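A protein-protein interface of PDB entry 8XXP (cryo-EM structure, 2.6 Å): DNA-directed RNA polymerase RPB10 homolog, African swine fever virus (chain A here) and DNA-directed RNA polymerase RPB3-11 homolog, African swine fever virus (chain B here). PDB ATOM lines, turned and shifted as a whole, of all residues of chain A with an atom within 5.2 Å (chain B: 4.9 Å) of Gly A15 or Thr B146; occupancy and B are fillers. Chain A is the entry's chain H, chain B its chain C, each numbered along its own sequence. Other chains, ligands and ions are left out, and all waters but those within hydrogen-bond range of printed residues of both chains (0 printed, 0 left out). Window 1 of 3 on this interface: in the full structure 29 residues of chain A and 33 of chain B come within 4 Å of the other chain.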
ATOM      1  N   ILE A   3      -7.278 -16.218 -22.374  1.00  0.00           N
ATOM      2  CA  ILE A   3      -6.413 -15.067 -22.644  1.00  0.00           C
ATOM      3  C   ILE A   3      -5.226 -15.545 -23.464  1.00  0.00           C
ATOM      4  O   ILE A   3      -4.616 -16.575 -23.122  1.00  0.00           O
ATOM      5  CB  ILE A   3      -5.953 -14.406 -21.335  1.00  0.00           C
ATOM      6  CG1 ILE A   3      -7.131 -13.735 -20.636  1.00  0.00           C
ATOM      7  CG2 ILE A   3      -4.876 -13.379 -21.597  1.00  0.00           C
ATOM      8  CD1 ILE A   3      -6.845 -13.338 -19.216  1.00  0.00           C
ATOM      9  N   PRO A   4      -4.867 -14.871 -24.552  1.00  0.00           N
ATOM     10  CA  PRO A   4      -3.820 -15.398 -25.427  1.00  0.00           C
ATOM     11  C   PRO A   4      -2.487 -15.501 -24.707  1.00  0.00           C
ATOM     12  O   PRO A   4      -2.224 -14.802 -23.730  1.00  0.00           O
ATOM     13  CB  PRO A   4      -3.768 -14.373 -26.564  1.00  0.00           C
ATOM     14  CG  PRO A   4      -4.334 -13.140 -25.975  1.00  0.00           C
ATOM     15  CD  PRO A   4      -5.401 -13.597 -25.055  1.00  0.00           C
ATOM     16  N   VAL A   5      -1.653 -16.420 -25.190  1.00  0.00           N
ATOM     17  CA  VAL A   5      -0.340 -16.625 -24.588  1.00  0.00           C
ATOM     18  C   VAL A   5       0.476 -15.342 -24.648  1.00  0.00           C
ATOM     19  O   VAL A   5       1.124 -14.951 -23.672  1.00  0.00           O
ATOM     20  CB  VAL A   5       0.381 -17.793 -25.279  1.00  0.00           C
ATOM     21  CG1 VAL A   5       1.785 -17.905 -24.773  1.00  0.00           C
ATOM     22  CG2 VAL A   5      -0.357 -19.075 -25.027  1.00  0.00           C
ATOM     23  N   VAL A   6       0.448 -14.661 -25.789  1.00  0.00           N
ATOM     24  CA  VAL A   6       1.140 -13.396 -25.970  1.00  0.00           C
ATOM     25  C   VAL A   6       0.118 -12.364 -26.414  1.00  0.00           C
ATOM     26  O   VAL A   6      -0.993 -12.696 -26.829  1.00  0.00           O
ATOM     27  CB  VAL A   6       2.285 -13.500 -26.996  1.00  0.00           C
ATOM     28  CG1 VAL A   6       3.373 -14.416 -26.486  1.00  0.00           C
ATOM     29  CG2 VAL A   6       1.759 -13.994 -28.311  1.00  0.00           C
ATOM     30  N   PRO A  13       4.414 -11.506 -23.656  1.00  0.00           N
ATOM     31  CA  PRO A  13       3.750 -12.692 -23.082  1.00  0.00           C
ATOM     32  C   PRO A  13       2.831 -12.396 -21.900  1.00  0.00           C
ATOM     33  O   PRO A  13       3.180 -12.523 -20.733  1.00  0.00           O
ATOM     34  CB  PRO A  13       4.935 -13.563 -22.667  1.00  0.00           C
ATOM     35  CG  PRO A  13       5.990 -12.586 -22.334  1.00  0.00           C
ATOM     36  CD  PRO A  13       5.842 -11.463 -23.308  1.00  0.00           C
ATOM     37  N   ILE A  14       1.600 -11.992 -22.209  1.00  0.00           N
ATOM     38  CA  ILE A  14       0.614 -11.761 -21.159  1.00  0.00           C
ATOM     39  C   ILE A  14       0.044 -13.066 -20.620  1.00  0.00           C
ATOM     40  O   ILE A  14      -0.536 -13.081 -19.526  1.00  0.00           O
ATOM     41  CB  ILE A  14      -0.510 -10.846 -21.673  1.00  0.00           C
ATOM     42  CG1 ILE A  14      -1.228 -11.487 -22.857  1.00  0.00           C
ATOM     43  CG2 ILE A  14       0.045  -9.497 -22.062  1.00  0.00           C
ATOM     44  CD1 ILE A  14      -2.313 -10.642 -23.437  1.00  0.00           C
ATOM     45  N   GLY A  15       0.196 -14.168 -21.354  1.00  0.00           N
ATOM     46  CA  GLY A  15      -0.268 -15.452 -20.866  1.00  0.00           C
ATOM     47  C   GLY A  15       0.535 -15.990 -19.707  1.00  0.00           C
ATOM     48  O   GLY A  15       0.079 -16.909 -19.023  1.00  0.00           O
ATOM     49  N   THR A  16       1.731 -15.448 -19.479  1.00  0.00           N
ATOM     50  CA  THR A  16       2.488 -15.793 -18.283  1.00  0.00           C
ATOM     51  C   THR A  16       1.714 -15.420 -17.031  1.00  0.00           C
ATOM     52  O   THR A  16       1.741 -16.142 -16.029  1.00  0.00           O
ATOM     53  CB  THR A  16       3.835 -15.077 -18.294  1.00  0.00           C
ATOM     54  OG1 THR A  16       4.314 -14.979 -19.638  1.00  0.00           O
ATOM     55  CG2 THR A  16       4.837 -15.833 -17.463  1.00  0.00           C
ATOM     56  N   TYR A  17       1.028 -14.287 -17.071  1.00  0.00           N
ATOM     57  CA  TYR A  17       0.268 -13.784 -15.946  1.00  0.00           C
ATOM     58  C   TYR A  17      -1.230 -13.883 -16.155  1.00  0.00           C
ATOM     59  O   TYR A  17      -1.979 -13.327 -15.359  1.00  0.00           O
ATOM     60  CB  TYR A  17       0.655 -12.331 -15.681  1.00  0.00           C
ATOM     61  CG  TYR A  17       2.141 -12.104 -15.742  1.00  0.00           C
ATOM     62  CD1 TYR A  17       2.993 -12.754 -14.867  1.00  0.00           C
ATOM     63  CD2 TYR A  17       2.697 -11.266 -16.696  1.00  0.00           C
ATOM     64  CE1 TYR A  17       4.349 -12.558 -14.922  1.00  0.00           C
ATOM     65  CE2 TYR A  17       4.055 -11.066 -16.761  1.00  0.00           C
ATOM     66  CZ  TYR A  17       4.876 -11.714 -15.869  1.00  0.00           C
ATOM     67  OH  TYR A  17       6.236 -11.520 -15.920  1.00  0.00           O
ATOM     68  N   ALA A  18      -1.682 -14.560 -17.212  1.00  0.00           N
ATOM     69  CA  ALA A  18      -3.111 -14.640 -17.502  1.00  0.00           C
ATOM     70  C   ALA A  18      -3.895 -15.262 -16.352  1.00  0.00           C
ATOM     71  O   ALA A  18      -4.924 -14.724 -15.927  1.00  0.00           O
ATOM     72  CB  ALA A  18      -3.331 -15.434 -18.787  1.00  0.00           C
ATOM     73  N   ALA A  19      -3.434 -16.403 -15.836  1.00  0.00           N
ATOM     74  CA  ALA A  19      -4.182 -17.099 -14.793  1.00  0.00           C
ATOM     75  C   ALA A  19      -4.176 -16.318 -13.485  1.00  0.00           C
ATOM     76  O   ALA A  19      -5.222 -16.166 -12.831  1.00  0.00           O
ATOM     77  CB  ALA A  19      -3.600 -18.493 -14.585  1.00  0.00           C
ATOM     78  N   ILE A  20      -3.002 -15.829 -13.084  1.00  0.00           N
ATOM     79  CA  ILE A  20      -2.905 -15.018 -11.878  1.00  0.00           C
ATOM     80  C   ILE A  20      -3.784 -13.788 -12.005  1.00  0.00           C
ATOM     81  O   ILE A  20      -4.484 -13.411 -11.062  1.00  0.00           O
ATOM     82  CB  ILE A  20      -1.440 -14.633 -11.604  1.00  0.00           C
ATOM     83  CG1 ILE A  20      -0.561 -15.877 -11.542  1.00  0.00           C
ATOM     84  CG2 ILE A  20      -1.337 -13.849 -10.324  1.00  0.00           C
ATOM     85  CD1 ILE A  20       0.908 -15.582 -11.649  1.00  0.00           C
ATOM     86  N   PHE B  30      -0.316 -21.450  -8.297  1.00  0.00           N
ATOM     87  CA  PHE B  30       0.951 -22.090  -8.614  1.00  0.00           C
ATOM     88  C   PHE B  30       1.862 -22.252  -7.410  1.00  0.00           C
ATOM     89  O   PHE B  30       3.001 -22.702  -7.577  1.00  0.00           O
ATOM     90  CB  PHE B  30       1.682 -21.290  -9.703  1.00  0.00           C
ATOM     91  CG  PHE B  30       0.831 -20.981 -10.897  1.00  0.00           C
ATOM     92  CD1 PHE B  30       0.568 -21.951 -11.844  1.00  0.00           C
ATOM     93  CD2 PHE B  30       0.268 -19.730 -11.055  1.00  0.00           C
ATOM     94  CE1 PHE B  30      -0.223 -21.674 -12.930  1.00  0.00           C
ATOM     95  CE2 PHE B  30      -0.526 -19.452 -12.139  1.00  0.00           C
ATOM     96  CZ  PHE B  30      -0.772 -20.422 -13.076  1.00  0.00           C
ATOM     97  N   LEU B  36       9.204 -15.560 -11.211  1.00  0.00           N
ATOM     98  CA  LEU B  36       9.222 -16.691 -12.110  1.00  0.00           C
ATOM     99  C   LEU B  36      10.643 -16.958 -12.593  1.00  0.00           C
ATOM    100  O   LEU B  36      11.486 -16.059 -12.594  1.00  0.00           O
ATOM    101  CB  LEU B  36       8.293 -16.430 -13.290  1.00  0.00           C
ATOM    102  CG  LEU B  36       6.816 -16.637 -12.978  1.00  0.00           C
ATOM    103  CD1 LEU B  36       5.956 -15.980 -14.025  1.00  0.00           C
ATOM    104  CD2 LEU B  36       6.514 -18.113 -12.890  1.00  0.00           C
ATOM    105  N   TYR B 126      -1.732 -26.455 -17.510  1.00  0.00           N
ATOM    106  CA  TYR B 126      -0.750 -25.395 -17.365  1.00  0.00           C
ATOM    107  C   TYR B 126       0.563 -25.813 -18.005  1.00  0.00           C
ATOM    108  O   TYR B 126       0.775 -26.977 -18.341  1.00  0.00           O
ATOM    109  CB  TYR B 126      -0.553 -25.034 -15.892  1.00  0.00           C
ATOM    110  CG  TYR B 126      -1.750 -24.342 -15.296  1.00  0.00           C
ATOM    111  CD1 TYR B 126      -2.038 -23.027 -15.608  1.00  0.00           C
ATOM    112  CD2 TYR B 126      -2.599 -25.008 -14.429  1.00  0.00           C
ATOM    113  CE1 TYR B 126      -3.133 -22.394 -15.071  1.00  0.00           C
ATOM    114  CE2 TYR B 126      -3.694 -24.383 -13.888  1.00  0.00           C
ATOM    115  CZ  TYR B 126      -3.957 -23.078 -14.212  1.00  0.00           C
ATOM    116  OH  TYR B 126      -5.051 -22.446 -13.676  1.00  0.00           O
ATOM    117  N   SER B 127       1.445 -24.833 -18.196  1.00  0.00           N
ATOM    118  CA  SER B 127       2.727 -25.115 -18.828  1.00  0.00           C
ATOM    119  C   SER B 127       3.602 -26.024 -17.980  1.00  0.00           C
ATOM    120  O   SER B 127       4.486 -26.689 -18.523  1.00  0.00           O
ATOM    121  CB  SER B 127       3.464 -23.816 -19.125  1.00  0.00           C
ATOM    122  OG  SER B 127       4.287 -23.962 -20.263  1.00  0.00           O
ATOM    123  N   ASN B 144       8.235 -20.649 -18.555  1.00  0.00           N
ATOM    124  CA  ASN B 144       7.558 -20.520 -17.278  1.00  0.00           C
ATOM    125  C   ASN B 144       6.450 -21.562 -17.155  1.00  0.00           C
ATOM    126  O   ASN B 144       5.885 -22.001 -18.157  1.00  0.00           O
ATOM    127  CB  ASN B 144       6.977 -19.120 -17.119  1.00  0.00           C
ATOM    128  CG  ASN B 144       8.029 -18.094 -16.781  1.00  0.00           C
ATOM    129  OD1 ASN B 144       8.937 -18.359 -16.007  1.00  0.00           O
ATOM    130  ND2 ASN B 144       7.912 -16.916 -17.365  1.00  0.00           N
ATOM    131  N   PRO B 145       6.121 -21.979 -15.933  1.00  0.00           N
ATOM    132  CA  PRO B 145       5.076 -22.989 -15.734  1.00  0.00           C
ATOM    133  C   PRO B 145       3.658 -22.446 -15.644  1.00  0.00           C
ATOM    134  O   PRO B 145       2.733 -23.232 -15.423  1.00  0.00           O
ATOM    135  CB  PRO B 145       5.489 -23.608 -14.397  1.00  0.00           C
ATOM    136  CG  PRO B 145       6.065 -22.468 -13.653  1.00  0.00           C
ATOM    137  CD  PRO B 145       6.787 -21.628 -14.667  1.00  0.00           C
ATOM    138  N   THR B 146       3.459 -21.144 -15.805  1.00  0.00           N
ATOM    139  CA  THR B 146       2.181 -20.513 -15.522  1.00  0.00           C
ATOM    140  C   THR B 146       1.323 -20.287 -16.757  1.00  0.00           C
ATOM    141  O   THR B 146       0.247 -19.696 -16.640  1.00  0.00           O
ATOM    142  CB  THR B 146       2.412 -19.186 -14.805  1.00  0.00           C
ATOM    143  OG1 THR B 146       3.133 -18.299 -15.665  1.00  0.00           O
ATOM    144  CG2 THR B 146       3.216 -19.410 -13.552  1.00  0.00           C
ATOM    145  N   PHE B 147       1.758 -20.734 -17.928  1.00  0.00           N
ATOM    146  CA  PHE B 147       0.945 -20.582 -19.124  1.00  0.00           C
ATOM    147  C   PHE B 147      -0.233 -21.539 -19.092  1.00  0.00           C
ATOM    148  O   PHE B 147      -0.101 -22.692 -18.684  1.00  0.00           O
ATOM    149  CB  PHE B 147       1.781 -20.837 -20.371  1.00  0.00           C
ATOM    150  CG  PHE B 147       2.776 -19.767 -20.654  1.00  0.00           C
ATOM    151  CD1 PHE B 147       2.414 -18.643 -21.367  1.00  0.00           C
ATOM    152  CD2 PHE B 147       4.071 -19.877 -20.204  1.00  0.00           C
ATOM    153  CE1 PHE B 147       3.324 -17.658 -21.626  1.00  0.00           C
ATOM    154  CE2 PHE B 147       4.984 -18.894 -20.460  1.00  0.00           C
ATOM    155  CZ  PHE B 147       4.610 -17.782 -21.170  1.00  0.00           C
ATOM    156  N   GLU B 148      -1.392 -21.056 -19.524  1.00  0.00           N
ATOM    157  CA  GLU B 148      -2.583 -21.888 -19.656  1.00  0.00           C
ATOM    158  C   GLU B 148      -2.564 -22.492 -21.052  1.00  0.00           C
ATOM    159  O   GLU B 148      -2.913 -21.829 -22.028  1.00  0.00           O
ATOM    160  CB  GLU B 148      -3.851 -21.074 -19.438  1.00  0.00           C
ATOM    161  CG  GLU B 148      -3.983 -20.427 -18.082  1.00  0.00           C
ATOM    162  CD  GLU B 148      -5.228 -19.571 -17.981  1.00  0.00           C
ATOM    163  OE1 GLU B 148      -5.422 -18.691 -18.846  1.00  0.00           O
ATOM    164  OE2 GLU B 148      -6.021 -19.780 -17.041  1.00  0.00           O
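The backbone carbonyl oxygen of Thr A16 sits at hydrogen-bond distance from the side-chain hydroxyl of Thr B146, at 2.6 Å.
The side-chain hydroxyl of Ser B127 sits close to the backbone carbonyl oxygen of Asn B144 (3.3 Å). The backbone NH (N) of Ser B127 is in hydrogen-bond range of the backbone carbonyl oxygen (O) of Phe B147 (2.7 Å). O of Pro A4 sits at hydrogen-bond distance from N of Gly A15 (3.5 Å). The backbone NH (N) of Ile A14 sits at hydrogen-bond distance from the backbone carbonyl oxygen (O) of Val A5 (3.3 Å). The backbone carbonyl oxygen of Val A5 sits at hydrogen-bond distance from the backbone NH of Gly A15, at 2.6 Å. The backbone carbonyl oxygen (O) of Pro A13 is in hydrogen-bond range of the side-chain hydroxyl (OG1) of Thr A16 (2.9 Å).
Among the printed residues, merely in contact across the chains: Val A5 with Phe B147 (3.5 Å), Gly A15 with Thr B146 (3.7 Å), Gly A15 with Phe B147 (3.7 Å), Thr A16 with Leu B36 (3.6 Å), Thr A16 with Asn B144 (3.3 Å), Thr A16 with Phe B147 (3.2 Å), Tyr A17 with Leu B36 (3.9 Å), Ala A18 with Glu B148 (3.9 Å), Ala A19 with Phe B30 (3.7 Å), Ala A19 with Tyr B126 (3.96 Å), Ala A19 with Glu B148 (3.7 Å) and Ile A20 with Phe B30 (3.6 Å).
Pro A4 touches none of the printed residues of chain B. Of the printed residues of chain B, Val A5 touches Phe B147. Gly A15 touches just these residues of chain B: Thr B146 (3.7 Å) and Phe B147 (3.7 Å). Printed residues of chain B within 4 Å of Tyr A17: Leu B36 (3.9 Å). Printed residues of chain A within 4 Å of Phe B30: Ala A19 and Ile A20. Printed residues of chain A within 4 Å of Leu B36: Thr A16 and Tyr A17. Of chain A, only Gly A15 (3.7 Å) and Thr A16 (2.6 Å) come within 4 Å of Thr B146. The nearest residue of chain B that does not touch Gly A15 is Glu B148 (4.4 Å). The nearest residue of chain A that does not touch Thr B146 is Ala A19 (4.5 Å). The nearest printed residue of chain A that does not touch Leu B36 is Ile A20 (5.6 Å).
Of the 12 printed residues of chain A, 7 touch a printed residue of chain B. Printed residues of chain A that touch a printed residue of chain B: Val A5, Gly A15, Thr A16, Tyr A17, Ala A18, Ala A19 and Ile A20. Hydrophobic or aromatic side chains of chain A within 4 Å of the printed part of chain B: Val A5, Tyr A17, Ala A18, Ala A19 and Ile A20. Of the 9 printed residues of chain B, 7 touch a printed residue of chain A. Printed residues of chain B that touch a printed residue of chain A: Phe B30, Leu B36, Tyr B126, Asn B144, Thr B146, Phe B147 and Glu B148. Among the printed residues, 13 pairs touch across the chains.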
